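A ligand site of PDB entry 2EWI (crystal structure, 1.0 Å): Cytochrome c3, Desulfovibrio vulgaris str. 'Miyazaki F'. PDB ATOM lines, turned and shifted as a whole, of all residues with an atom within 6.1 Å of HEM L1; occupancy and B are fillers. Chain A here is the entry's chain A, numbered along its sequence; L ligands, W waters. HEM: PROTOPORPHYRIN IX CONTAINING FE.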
ATOM      1  N   MET A  11      21.347   3.058  34.431  1.00  0.00           N
ATOM      2  CA  MET A  11      20.772   3.119  33.122  1.00  0.00           C
ATOM      3  C   MET A  11      20.601   1.669  32.657  1.00  0.00           C
ATOM      4  O   MET A  11      21.606   0.949  32.531  1.00  0.00           O
ATOM      5  CB  MET A  11      21.719   3.912  32.187  1.00  0.00           C
ATOM      6  CG  MET A  11      21.938   5.352  32.687  1.00  0.00           C
ATOM      7  SD  MET A  11      23.136   6.242  31.666  1.00  0.00           S
ATOM      8  CE  MET A  11      22.152   6.580  30.216  1.00  0.00           C
ATOM      9  N   ASP A  12      19.347   1.267  32.518  1.00  0.00           N
ATOM     10  CA  ASP A  12      19.067  -0.181  32.319  1.00  0.00           C
ATOM     11  C   ASP A  12      17.962  -0.414  31.325  1.00  0.00           C
ATOM     12  O   ASP A  12      17.158  -1.363  31.473  1.00  0.00           O
ATOM     13  CB  ASP A  12      18.835  -0.883  33.677  1.00  0.00           C
ATOM     14  CG  ASP A  12      17.749  -0.240  34.454  1.00  0.00           C
ATOM     15  OD1 ASP A  12      16.913   0.563  33.940  1.00  0.00           O
ATOM     16  OD2 ASP A  12      17.716  -0.494  35.716  1.00  0.00           O
ATOM     17  N   LYS A  13      17.983   0.357  30.249  1.00  0.00           N
ATOM     18  CA  LYS A  13      17.111   0.066  29.119  1.00  0.00           C
ATOM     19  C   LYS A  13      17.536  -1.184  28.342  1.00  0.00           C
ATOM     20  O   LYS A  13      16.717  -1.674  27.537  1.00  0.00           O
ATOM     21  CB  LYS A  13      17.125   1.221  28.129  1.00  0.00           C
ATOM     22  CG  LYS A  13      16.783   2.567  28.730  1.00  0.00           C
ATOM     23  CD  LYS A  13      15.468   2.687  29.473  1.00  0.00           C
ATOM     24  CE  LYS A  13      14.308   2.390  28.607  1.00  0.00           C
ATOM     25  NZ  LYS A  13      13.022   2.793  29.267  1.00  0.00           N
ATOM     26  N   THR A  14      18.753  -1.638  28.549  1.00  0.00           N
ATOM     27  CA  THR A  14      19.380  -2.725  27.779  1.00  0.00           C
ATOM     28  C   THR A  14      19.887  -3.823  28.697  1.00  0.00           C
ATOM     29  O   THR A  14      19.845  -3.669  29.910  1.00  0.00           O
ATOM     30  CB  THR A  14      20.558  -2.197  26.912  1.00  0.00           C
ATOM     31  OG1 THR A  14      21.723  -2.130  27.749  1.00  0.00           O
ATOM     32  CG2 THR A  14      20.256  -0.862  26.259  1.00  0.00           C
ATOM     33  N   LYS A  15      20.361  -4.898  28.103  1.00  0.00           N
ATOM     34  CA  LYS A  15      20.981  -5.990  28.841  1.00  0.00           C
ATOM     35  C   LYS A  15      22.442  -5.712  29.230  1.00  0.00           C
ATOM     36  O   LYS A  15      23.094  -6.577  29.842  1.00  0.00           O
ATOM     37  CB  LYS A  15      20.864  -7.320  28.086  1.00  0.00           C
ATOM     38  CG  LYS A  15      19.378  -7.731  28.041  1.00  0.00           C
ATOM     39  CD  LYS A  15      19.283  -9.126  27.429  1.00  0.00           C
ATOM     40  CE  LYS A  15      17.857  -9.496  27.077  1.00  0.00           C
ATOM     41  NZ  LYS A  15      17.745 -10.851  26.467  1.00  0.00           N
ATOM     42  N   GLN A  16      22.910  -4.485  28.948  1.00  0.00           N
ATOM     43  CA  GLN A  16      24.236  -4.072  29.353  1.00  0.00           C
ATOM     44  C   GLN A  16      24.143  -2.792  30.187  1.00  0.00           C
ATOM     45  O   GLN A  16      24.569  -1.732  29.785  1.00  0.00           O
ATOM     46  CB  GLN A  16      25.137  -3.858  28.158  1.00  0.00           C
ATOM     47  CG  GLN A  16      25.169  -5.044  27.168  1.00  0.00           C
ATOM     48  CD  GLN A  16      25.590  -6.376  27.713  1.00  0.00           C
ATOM     49  OE1 GLN A  16      26.312  -6.433  28.680  1.00  0.00           O
ATOM     50  NE2 GLN A  16      25.087  -7.396  27.030  1.00  0.00           N
ATOM     51  N   PRO A  17      23.518  -2.876  31.346  1.00  0.00           N
ATOM     52  CA  PRO A  17      23.232  -1.665  32.131  1.00  0.00           C
ATOM     53  C   PRO A  17      24.519  -1.006  32.633  1.00  0.00           C
ATOM     54  O   PRO A  17      25.554  -1.643  32.897  1.00  0.00           O
ATOM     55  CB  PRO A  17      22.428  -2.205  33.334  1.00  0.00           C
ATOM     56  CG  PRO A  17      22.806  -3.646  33.426  1.00  0.00           C
ATOM     57  CD  PRO A  17      23.010  -4.098  32.019  1.00  0.00           C
ATOM     58  N   VAL A  18      24.399   0.332  32.830  1.00  0.00           N
ATOM     59  CA  VAL A  18      25.565   1.164  33.178  1.00  0.00           C
ATOM     60  C   VAL A  18      25.177   2.112  34.312  1.00  0.00           C
ATOM     61  O   VAL A  18      24.114   2.717  34.257  1.00  0.00           O
ATOM     62  CB  VAL A  18      26.044   1.976  31.953  1.00  0.00           C
ATOM     63  CG1 VAL A  18      27.152   2.943  32.301  1.00  0.00           C
ATOM     64  CG2 VAL A  18      26.540   1.014  30.864  1.00  0.00           C
ATOM     65  N   MET A  55      15.543   1.275  20.351  1.00  0.00           N
ATOM     66  CA  MET A  55      16.443   0.335  20.959  1.00  0.00           C
ATOM     67  C   MET A  55      17.173  -0.600  20.005  1.00  0.00           C
ATOM     68  O   MET A  55      17.752  -1.607  20.427  1.00  0.00           O
ATOM     69  CB  MET A  55      15.635  -0.421  22.043  1.00  0.00           C
ATOM     70  CG  MET A  55      15.225   0.493  23.190  1.00  0.00           C
ATOM     71  SD  MET A  55      16.656   1.065  24.164  1.00  0.00           S
ATOM     72  CE  MET A  55      16.056   2.609  24.783  1.00  0.00           C
ATOM     73  N   ASP A  56      17.146  -0.243  18.717  1.00  0.00           N
ATOM     74  CA  ASP A  56      18.030  -0.928  17.759  1.00  0.00           C
ATOM     75  C   ASP A  56      19.411  -0.275  17.806  1.00  0.00           C
ATOM     76  O   ASP A  56      19.555   0.886  17.437  1.00  0.00           O
ATOM     77  CB  ASP A  56      17.411  -0.847  16.382  1.00  0.00           C
ATOM     78  CG  ASP A  56      18.206  -1.100  15.193  1.00  0.00           C
ATOM     79  OD1 ASP A  56      17.708  -0.768  14.061  1.00  0.00           O
ATOM     80  OD2 ASP A  56      19.360  -1.439  15.193  1.00  0.00           O
ATOM     81  N   LYS A  57      20.391  -1.031  18.254  1.00  0.00           N
ATOM     82  CA  LYS A  57      21.728  -0.502  18.512  1.00  0.00           C
ATOM     83  C   LYS A  57      22.490  -0.129  17.243  1.00  0.00           C
ATOM     84  O   LYS A  57      23.532   0.508  17.389  1.00  0.00           O
ATOM     85  CB  LYS A  57      22.493  -1.418  19.463  1.00  0.00           C
ATOM     86  CG  LYS A  57      23.004  -2.694  18.748  1.00  0.00           C
ATOM     87  CD  LYS A  57      23.865  -3.532  19.710  1.00  0.00           C
ATOM     88  CE  LYS A  57      24.002  -4.985  19.230  1.00  0.00           C
ATOM     89  NZ  LYS A  57      24.956  -5.667  20.140  1.00  0.00           N
ATOM     90  N   TYR A  65      19.083   5.098  20.779  1.00  0.00           N
ATOM     91  CA  TYR A  65      19.601   5.170  22.174  1.00  0.00           C
ATOM     92  C   TYR A  65      21.099   4.812  22.230  1.00  0.00           C
ATOM     93  O   TYR A  65      21.895   5.543  22.825  1.00  0.00           O
ATOM     94  CB  TYR A  65      18.747   4.261  23.035  1.00  0.00           C
ATOM     95  CG  TYR A  65      19.092   4.223  24.496  1.00  0.00           C
ATOM     96  CD1 TYR A  65      19.764   3.143  25.045  1.00  0.00           C
ATOM     97  CD2 TYR A  65      18.742   5.287  25.333  1.00  0.00           C
ATOM     98  CE1 TYR A  65      20.031   3.128  26.409  1.00  0.00           C
ATOM     99  CE2 TYR A  65      19.031   5.252  26.686  1.00  0.00           C
ATOM    100  CZ  TYR A  65      19.701   4.162  27.213  1.00  0.00           C
ATOM    101  OH  TYR A  65      20.005   4.153  28.576  1.00  0.00           O
ATOM    102  N   TYR A  66      21.476   3.681  21.630  1.00  0.00           N
ATOM    103  CA  TYR A  66      22.882   3.287  21.616  1.00  0.00           C
ATOM    104  C   TYR A  66      23.713   4.412  21.004  1.00  0.00           C
ATOM    105  O   TYR A  66      24.786   4.782  21.515  1.00  0.00           O
ATOM    106  CB  TYR A  66      23.056   1.973  20.813  1.00  0.00           C
ATOM    107  CG  TYR A  66      24.487   1.525  20.749  1.00  0.00           C
ATOM    108  CD1 TYR A  66      25.397   2.017  19.811  1.00  0.00           C
ATOM    109  CD2 TYR A  66      24.983   0.563  21.639  1.00  0.00           C
ATOM    110  CE1 TYR A  66      26.694   1.628  19.730  1.00  0.00           C
ATOM    111  CE2 TYR A  66      26.329   0.141  21.568  1.00  0.00           C
ATOM    112  CZ  TYR A  66      27.165   0.687  20.623  1.00  0.00           C
ATOM    113  OH  TYR A  66      28.474   0.260  20.553  1.00  0.00           O
ATOM    114  N   MET A  69      24.715   7.302  23.220  1.00  0.00           N
ATOM    115  CA  MET A  69      25.651   7.031  24.301  1.00  0.00           C
ATOM    116  C   MET A  69      27.061   6.692  23.779  1.00  0.00           C
ATOM    117  O   MET A  69      28.015   6.840  24.565  1.00  0.00           O
ATOM    118  CB  MET A  69      25.179   5.868  25.186  1.00  0.00           C
ATOM    119  CG  MET A  69      23.759   6.003  25.700  1.00  0.00           C
ATOM    120  SD  MET A  69      23.520   7.564  26.622  1.00  0.00           S
ATOM    121  CE  MET A  69      21.711   7.609  26.649  1.00  0.00           C
ATOM    122  N   HIS A  70      27.223   6.290  22.525  1.00  0.00           N
ATOM    123  CA  HIS A  70      28.483   5.733  22.064  1.00  0.00           C
ATOM    124  C   HIS A  70      29.158   6.460  20.916  1.00  0.00           C
ATOM    125  O   HIS A  70      30.377   6.269  20.756  1.00  0.00           O
ATOM    126  CB  HIS A  70      28.279   4.255  21.607  1.00  0.00           C
ATOM    127  CG  HIS A  70      27.889   3.339  22.707  1.00  0.00           C
ATOM    128  ND1 HIS A  70      26.551   3.199  23.061  1.00  0.00           N
ATOM    129  CD2 HIS A  70      28.571   2.535  23.545  1.00  0.00           C
ATOM    130  CE1 HIS A  70      26.478   2.331  24.086  1.00  0.00           C
ATOM    131  NE2 HIS A  70      27.691   1.900  24.395  1.00  0.00           N
ATOM    132  N   CYS A  79      28.539   9.844  25.779  1.00  0.00           N
ATOM    133  CA  CYS A  79      29.392   9.326  26.860  1.00  0.00           C
ATOM    134  C   CYS A  79      30.781   8.932  26.293  1.00  0.00           C
ATOM    135  O   CYS A  79      31.823   9.359  26.782  1.00  0.00           O
ATOM    136  CB  CYS A  79      28.786   8.059  27.486  1.00  0.00           C
ATOM    137  SG  CYS A  79      27.035   8.023  27.920  1.00  0.00           S
ATOM    138  N   VAL A  80      30.766   8.071  25.276  1.00  0.00           N
ATOM    139  CA  VAL A  80      32.036   7.565  24.734  1.00  0.00           C
ATOM    140  C   VAL A  80      32.783   8.662  24.008  1.00  0.00           C
ATOM    141  O   VAL A  80      34.025   8.775  24.137  1.00  0.00           O
ATOM    142  CB  VAL A  80      31.818   6.312  23.857  1.00  0.00           C
ATOM    143  CG1 VAL A  80      33.165   5.849  23.261  1.00  0.00           C
ATOM    144  CG2 VAL A  80      31.207   5.189  24.680  1.00  0.00           C
ATOM    145  N   HIS A  83      34.454  10.833  26.511  1.00  0.00           N
ATOM    146  CA  HIS A  83      35.535  10.065  27.178  1.00  0.00           C
ATOM    147  C   HIS A  83      36.741   9.861  26.268  1.00  0.00           C
ATOM    148  O   HIS A  83      37.867   9.826  26.791  1.00  0.00           O
ATOM    149  CB  HIS A  83      34.978   8.723  27.667  1.00  0.00           C
ATOM    150  CG  HIS A  83      34.096   8.882  28.884  1.00  0.00           C
ATOM    151  ND1 HIS A  83      33.819   7.745  29.627  1.00  0.00           N
ATOM    152  CD2 HIS A  83      33.513   9.907  29.520  1.00  0.00           C
ATOM    153  CE1 HIS A  83      33.050   8.107  30.631  1.00  0.00           C
ATOM    154  NE2 HIS A  83      32.794   9.407  30.634  1.00  0.00           N
ATOM    155  N   GLU A  96      39.843   2.380  30.684  1.00  0.00           N
ATOM    156  CA  GLU A  96      38.933   2.694  31.763  1.00  0.00           C
ATOM    157  C   GLU A  96      37.663   3.424  31.320  1.00  0.00           C
ATOM    158  O   GLU A  96      36.552   3.152  31.817  1.00  0.00           O
ATOM    159  CB  GLU A  96      39.687   3.582  32.754  1.00  0.00           C
ATOM    160  CG  GLU A  96      39.181   3.893  34.117  1.00  0.00           C
ATOM    161  CD  GLU A  96      40.284   4.729  34.801  1.00  0.00           C
ATOM    162  OE1 GLU A  96      39.993   5.879  35.093  1.00  0.00           O
ATOM    163  OE2 GLU A  96      41.414   4.204  34.931  1.00  0.00           O
ATOM    164  N   LEU A  97      37.826   4.393  30.429  1.00  0.00           N
ATOM    165  CA  LEU A  97      36.764   5.315  30.113  1.00  0.00           C
ATOM    166  C   LEU A  97      36.075   4.979  28.802  1.00  0.00           C
ATOM    167  O   LEU A  97      34.945   5.461  28.579  1.00  0.00           O
ATOM    168  CB  LEU A  97      37.345   6.743  30.028  1.00  0.00           C
ATOM    169  CG  LEU A  97      37.914   7.295  31.332  1.00  0.00           C
ATOM    170  CD1 LEU A  97      38.436   8.727  31.053  1.00  0.00           C
ATOM    171  CD2 LEU A  97      36.921   7.285  32.464  1.00  0.00           C
ATOM    172  N   THR A  98      36.697   4.200  27.901  1.00  0.00           N
ATOM    173  CA  THR A  98      36.121   3.956  26.596  1.00  0.00           C
ATOM    174  C   THR A  98      36.065   2.467  26.223  1.00  0.00           C
ATOM    175  O   THR A  98      35.475   2.151  25.202  1.00  0.00           O
ATOM    176  CB  THR A  98      36.796   4.727  25.434  1.00  0.00           C
ATOM    177  OG1 THR A  98      38.104   4.203  25.133  1.00  0.00           O
ATOM    178  CG2 THR A  98      36.900   6.184  25.816  1.00  0.00           C
ATOM    179  N   GLY A  99      36.649   1.576  27.029  1.00  0.00           N
ATOM    180  CA  GLY A  99      36.656   0.179  26.680  1.00  0.00           C
ATOM    181  C   GLY A  99      35.280  -0.400  26.654  1.00  0.00           C
ATOM    182  O   GLY A  99      34.379  -0.110  27.425  1.00  0.00           O
ATOM    183  N   CYS A 100      35.111  -1.336  25.681  1.00  0.00           N
ATOM    184  CA  CYS A 100      33.786  -1.937  25.524  1.00  0.00           C
ATOM    185  C   CYS A 100      33.498  -2.983  26.555  1.00  0.00           C
ATOM    186  O   CYS A 100      32.331  -3.349  26.799  1.00  0.00           O
ATOM    187  CB  CYS A 100      33.624  -2.556  24.115  1.00  0.00           C
ATOM    188  SG  CYS A 100      34.031  -1.440  22.773  1.00  0.00           S
ATOM    189  N   LYS A 101      34.550  -3.521  27.195  1.00  0.00           N
ATOM    190  CA  LYS A 101      34.413  -4.438  28.311  1.00  0.00           C
ATOM    191  C   LYS A 101      35.557  -4.123  29.261  1.00  0.00           C
ATOM    192  O   LYS A 101      36.503  -3.485  28.829  1.00  0.00           O
ATOM    193  CB  LYS A 101      34.416  -5.899  27.911  1.00  0.00           C
ATOM    194  CG  LYS A 101      35.692  -6.319  27.187  1.00  0.00           C
ATOM    195  CD  LYS A 101      35.572  -7.825  26.899  1.00  0.00           C
ATOM    196  CE  LYS A 101      36.952  -8.380  26.579  1.00  0.00           C
ATOM    197  NZ  LYS A 101      37.655  -8.671  27.848  1.00  0.00           N
ATOM    198  N   SER A 103      35.664  -1.891  31.447  1.00  0.00           N
ATOM    199  CA  SER A 103      35.796  -0.455  31.644  1.00  0.00           C
ATOM    200  C   SER A 103      34.953  -0.018  32.837  1.00  0.00           C
ATOM    201  O   SER A 103      34.243  -0.814  33.428  1.00  0.00           O
ATOM    202  CB  SER A 103      35.365   0.296  30.383  1.00  0.00           C
ATOM    203  OG  SER A 103      33.943   0.108  30.157  1.00  0.00           O
ATOM    204  N   LYS A 104      34.958   1.298  33.104  1.00  0.00           N
ATOM    205  CA  LYS A 104      34.112   1.813  34.182  1.00  0.00           C
ATOM    206  C   LYS A 104      32.637   1.846  33.775  1.00  0.00           C
ATOM    207  O   LYS A 104      31.775   1.998  34.638  1.00  0.00           O
ATOM    208  CB  LYS A 104      34.549   3.213  34.553  1.00  0.00           C
ATOM    209  CG  LYS A 104      35.967   3.258  35.102  1.00  0.00           C
ATOM    210  CD  LYS A 104      36.023   3.695  36.530  1.00  0.00           C
ATOM    211  CE  LYS A 104      37.446   3.716  37.062  1.00  0.00           C
ATOM    212  NZ  LYS A 104      37.418   3.438  38.522  1.00  0.00           N
ATOM    213  N   CYS A 105      32.341   1.687  32.489  1.00  0.00           N
ATOM    214  CA  CYS A 105      30.936   1.560  32.052  1.00  0.00           C
ATOM    215  C   CYS A 105      30.454   0.112  32.034  1.00  0.00           C
ATOM    216  O   CYS A 105      29.395  -0.194  32.550  1.00  0.00           O
ATOM    217  CB  CYS A 105      30.704   2.180  30.677  1.00  0.00           C
ATOM    218  SG  CYS A 105      31.108   3.956  30.755  1.00  0.00           S
ATOM    219  N   HIS A 106      31.224  -0.765  31.386  1.00  0.00           N
ATOM    220  CA  HIS A 106      30.836  -2.166  31.159  1.00  0.00           C
ATOM    221  C   HIS A 106      31.873  -3.111  31.792  1.00  0.00           C
ATOM    222  O   HIS A 106      33.028  -3.088  31.431  1.00  0.00           O
ATOM    223  CB  HIS A 106      30.775  -2.470  29.668  1.00  0.00           C
ATOM    224  CG  HIS A 106      29.714  -1.731  28.914  1.00  0.00           C
ATOM    225  ND1 HIS A 106      28.367  -1.779  29.210  1.00  0.00           N
ATOM    226  CD2 HIS A 106      29.802  -0.935  27.806  1.00  0.00           C
ATOM    227  CE1 HIS A 106      27.700  -1.026  28.294  1.00  0.00           C
ATOM    228  NE2 HIS A 106      28.557  -0.533  27.451  1.00  0.00           N
HETATM  229  CHA HEM L   1      24.812  -0.042  26.325  1.00  0.00           C
HETATM  230  CHB HEM L   1      28.386  -1.878  23.711  1.00  0.00           C
HETATM  231  CHC HEM L   1      31.510   1.257  25.576  1.00  0.00           C
HETATM  232  CHD HEM L   1      27.829   3.337  27.968  1.00  0.00           C
HETATM  233  C1A HEM L   1      25.547  -0.914  25.509  1.00  0.00           C
HETATM  234  C2A HEM L   1      25.025  -2.068  24.886  1.00  0.00           C
HETATM  235  C3A HEM L   1      26.054  -2.567  24.131  1.00  0.00           C
HETATM  236  C4A HEM L   1      27.144  -1.745  24.365  1.00  0.00           C
HETATM  237  CMA HEM L   1      26.005  -3.806  23.226  1.00  0.00           C
HETATM  238  CAA HEM L   1      23.582  -2.564  24.865  1.00  0.00           C
HETATM  239  CBA HEM L   1      22.855  -2.132  23.617  1.00  0.00           C
HETATM  240  CGA HEM L   1      21.513  -2.834  23.439  1.00  0.00           C
HETATM  241  O1A HEM L   1      21.477  -4.084  23.550  1.00  0.00           O
HETATM  242  O2A HEM L   1      20.494  -2.160  23.229  1.00  0.00           O
HETATM  243  C1B HEM L   1      29.506  -1.068  23.836  1.00  0.00           C
HETATM  244  C2B HEM L   1      30.668  -1.177  23.054  1.00  0.00           C
HETATM  245  C3B HEM L   1      31.592  -0.295  23.605  1.00  0.00           C
HETATM  246  C4B HEM L   1      30.899   0.317  24.698  1.00  0.00           C
HETATM  247  CMB HEM L   1      30.848  -2.089  21.861  1.00  0.00           C
HETATM  248  CAB HEM L   1      32.960   0.028  23.163  1.00  0.00           C
HETATM  249  CBB HEM L   1      33.005   0.844  21.935  1.00  0.00           C
HETATM  250  C1C HEM L   1      30.769   1.999  26.535  1.00  0.00           C
HETATM  251  C2C HEM L   1      31.359   2.894  27.436  1.00  0.00           C
HETATM  252  C3C HEM L   1      30.310   3.532  28.113  1.00  0.00           C
HETATM  253  C4C HEM L   1      29.138   2.954  27.582  1.00  0.00           C
HETATM  254  CMC HEM L   1      32.850   3.084  27.605  1.00  0.00           C
HETATM  255  CAC HEM L   1      30.394   4.581  29.157  1.00  0.00           C
HETATM  256  CBC HEM L   1      31.243   5.784  28.777  1.00  0.00           C
HETATM  257  C1D HEM L   1      26.657   2.660  27.615  1.00  0.00           C
HETATM  258  C2D HEM L   1      25.374   3.052  28.078  1.00  0.00           C
HETATM  259  C3D HEM L   1      24.514   2.054  27.657  1.00  0.00           C
HETATM  260  C4D HEM L   1      25.297   1.117  26.963  1.00  0.00           C
HETATM  261  CMD HEM L   1      25.058   4.276  28.887  1.00  0.00           C
HETATM  262  CAD HEM L   1      23.020   1.928  27.962  1.00  0.00           C
HETATM  263  CBD HEM L   1      22.748   1.233  29.302  1.00  0.00           C
HETATM  264  CGD HEM L   1      21.296   0.849  29.475  1.00  0.00           C
HETATM  265  O1D HEM L   1      20.426   1.762  29.476  1.00  0.00           O
HETATM  266  O2D HEM L   1      21.025  -0.375  29.611  1.00  0.00           O
HETATM  267  NA  HEM L   1      26.844  -0.735  25.209  1.00  0.00           N
HETATM  268  NB  HEM L   1      29.643  -0.108  24.793  1.00  0.00           N
HETATM  269  NC  HEM L   1      29.407   2.002  26.663  1.00  0.00           N
HETATM  270  ND  HEM L   1      26.603   1.498  26.918  1.00  0.00           N
HETATM  271 FE   HEM L   1      28.120   0.658  25.899  1.00  0.00          FE
HETATM  272  CHA HEM L   2      34.127   9.811  34.263  1.00  0.00           C
HETATM  273  CHB HEM L   2      30.257   7.358  32.757  1.00  0.00           C
HETATM  274  CHC HEM L   2      29.161  11.068  29.842  1.00  0.00           C
HETATM  275  CHD HEM L   2      33.296  13.254  30.982  1.00  0.00           C
HETATM  276  C1A HEM L   2      33.136   8.814  34.136  1.00  0.00           C
HETATM  277  C2A HEM L   2      33.184   7.612  34.827  1.00  0.00           C
HETATM  278  C3A HEM L   2      32.092   6.900  34.396  1.00  0.00           C
HETATM  279  C4A HEM L   2      31.442   7.722  33.453  1.00  0.00           C
HETATM  280  CMA HEM L   2      31.578   5.497  34.774  1.00  0.00           C
HETATM  281  CAA HEM L   2      34.216   7.211  35.905  1.00  0.00           C
HETATM  282  CBA HEM L   2      33.837   7.882  37.260  1.00  0.00           C
HETATM  283  CGA HEM L   2      32.526   7.326  37.794  1.00  0.00           C
HETATM  284  O1A HEM L   2      32.496   6.115  38.178  1.00  0.00           O
HETATM  285  O2A HEM L   2      31.526   8.077  37.848  1.00  0.00           O
HETATM  286  C1B HEM L   2      29.633   8.170  31.803  1.00  0.00           C
HETATM  287  C2B HEM L   2      28.408   7.812  31.144  1.00  0.00           C
HETATM  288  C3B HEM L   2      28.058   8.873  30.357  1.00  0.00           C
HETATM  289  C4B HEM L   2      29.106   9.834  30.543  1.00  0.00           C
HETATM  290  CMB HEM L   2      27.704   6.470  31.320  1.00  0.00           C
HETATM  291  CAB HEM L   2      26.911   9.061  29.468  1.00  0.00           C
HETATM  292  CBB HEM L   2      25.561   8.783  30.094  1.00  0.00           C
HETATM  293  C1C HEM L   2      30.239  11.973  29.857  1.00  0.00           C
HETATM  294  C2C HEM L   2      30.308  13.104  28.994  1.00  0.00           C
HETATM  295  C3C HEM L   2      31.515  13.733  29.284  1.00  0.00           C
HETATM  296  C4C HEM L   2      32.087  12.955  30.327  1.00  0.00           C
HETATM  297  CMC HEM L   2      29.241  13.454  27.963  1.00  0.00           C
HETATM  298  CAC HEM L   2      32.105  14.941  28.707  1.00  0.00           C
HETATM  299  CBC HEM L   2      31.245  15.951  28.011  1.00  0.00           C
HETATM  300  C1D HEM L   2      33.867  12.521  32.033  1.00  0.00           C
HETATM  301  C2D HEM L   2      35.040  12.922  32.718  1.00  0.00           C
HETATM  302  C3D HEM L   2      35.260  11.949  33.685  1.00  0.00           C
HETATM  303  C4D HEM L   2      34.248  11.016  33.501  1.00  0.00           C
HETATM  304  CMD HEM L   2      35.853  14.152  32.419  1.00  0.00           C
HETATM  305  CAD HEM L   2      36.434  11.848  34.631  1.00  0.00           C
HETATM  306  CBD HEM L   2      37.536  11.044  33.972  1.00  0.00           C
HETATM  307  CGD HEM L   2      38.418  10.285  34.928  1.00  0.00           C
HETATM  308  O1D HEM L   2      39.533   9.955  34.503  1.00  0.00           O
HETATM  309  O2D HEM L   2      37.799   9.731  35.869  1.00  0.00           O
HETATM  310  NA  HEM L   2      32.103   8.886  33.274  1.00  0.00           N
HETATM  311  NB  HEM L   2      30.035   9.403  31.417  1.00  0.00           N
HETATM  312  NC  HEM L   2      31.330  11.865  30.617  1.00  0.00           N
HETATM  313  ND  HEM L   2      33.393  11.361  32.532  1.00  0.00           N
HETATM  314 FE   HEM L   2      31.729  10.386  31.964  1.00  0.00          FE
HETATM  315  O   HOH W   1      17.952  -2.786  22.885  1.00  0.00           O
HETATM  316  O   HOH W   2      23.192  -5.926  22.501  1.00  0.00           O
HETATM  317  O   HOH W   3      19.776   0.445  22.783  1.00  0.00           O
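The side-chain hydroxyl (OG1) of Thr 14 lies within hydrogen-bond range of an oxygen (O2D) of HEM L1. An iron atom (FE) of HEM L2 is bound by a ring nitrogen (NE2) of His 83 (2.0 Å). The backbone NH of Asp 12 is in hydrogen-bond range of an oxygen (O1D) of HEM L1 (3.3 Å). The side-chain sulfur (SG) of Cys 105 is covalently linked to a carbon (CAC) of HEM L1 (1.9 Å). NE2 of His 106 binds FE of HEM L1 (2.0 Å). The side-chain hydroxyl (OH) of Tyr 65 lies within hydrogen-bond range of an oxygen (O1D) of HEM L1. The backbone NH (N) of Thr 14 sits at hydrogen-bond distance from an oxygen (O2D) of HEM L1, at 2.8 Å. NE2 of His 70 binds FE of HEM L1. A carbon (CAB) of HEM L2 is bonded to the side-chain sulfur of Cys 79. SG of Cys 100 is bonded to CAB of HEM L1 (1.9 Å). N of Lys 13 sits at hydrogen-bond distance from O1D of HEM L1, 2.9 Å away.
Water W1 lies within hydrogen-bond range of an oxygen (O2A) of HEM L1 (2.6 Å) and the backbone carbonyl oxygen (O) of Met 55 (2.7 Å). Water W2 lies within hydrogen-bond range of an oxygen (O1A) of HEM L1 (2.7 Å) and the side-chain amino group (NZ) of Lys 57 (3.0 Å). Water W3 bridges an oxygen (O2A) of HEM L1 (2.7 Å) and the side-chain sulfur (SD) of Met 55 (3.5 Å).
N of Met 11 is in hydrogen-bond range of O of Val 18. O of Gly 99 lies within hydrogen-bond range of OG of Ser 103, 2.8 Å away. The backbone carbonyl oxygen (O) of Met 69 lies within hydrogen-bond range of the backbone NH (N) of Val 80, at 3.1 Å. The side-chain hydroxyl (OG1) of Thr 14 sits at hydrogen-bond distance from the backbone NH (N) of Gln 16. The backbone carbonyl oxygen (O) of Leu 97 sits at hydrogen-bond distance from a ring nitrogen (ND1) of His 83, at 2.8 Å. N of Cys 79 sits close to O of Met 69. The backbone NH of Cys 105 sits close to the side-chain hydroxyl of Ser 103. N of His 106 sits at hydrogen-bond distance from OG of Ser 103 (3.1 Å).
An oxygen (O2D) of HEM L1 sits close to the backbone carbonyl oxygen (O) of Met 11 (3.3 Å). Merely in contact with HEM L1: Leu 97 (3.3 Å), His 83 (3.3 Å), Tyr 66 (3.5 Å), Gln 16 (3.5 Å), Thr 98 (3.5 Å), Gly 99 (3.5 Å), Cys 79 (3.6 Å), Pro 17 (3.6 Å), Val 80 (3.6 Å), Val 18 (3.6 Å), Lys 57 (3.8 Å), Met 69 (3.9 Å) and Met 55 (3.96 Å). Hydrophobic or aromatic side chains that line HEM L1: Met 11, Val 18, Tyr 65, Tyr 66, Met 69, His 70, Val 80, His 83 and His 106. 22 residues have an atom within 4 Å of HEM L1: Met 11, Asp 12, Lys 13, Thr 14, Gln 16, Pro 17, Val 18, Met 55, Lys 57, Tyr 65, Tyr 66, Met 69, His 70, Cys 79, Val 80, His 83, Leu 97, Thr 98, Gly 99, Cys 100, Cys 105 and His 106. Along chain A the residues within 4 Å of HEM L1 span positions 11 to 106.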
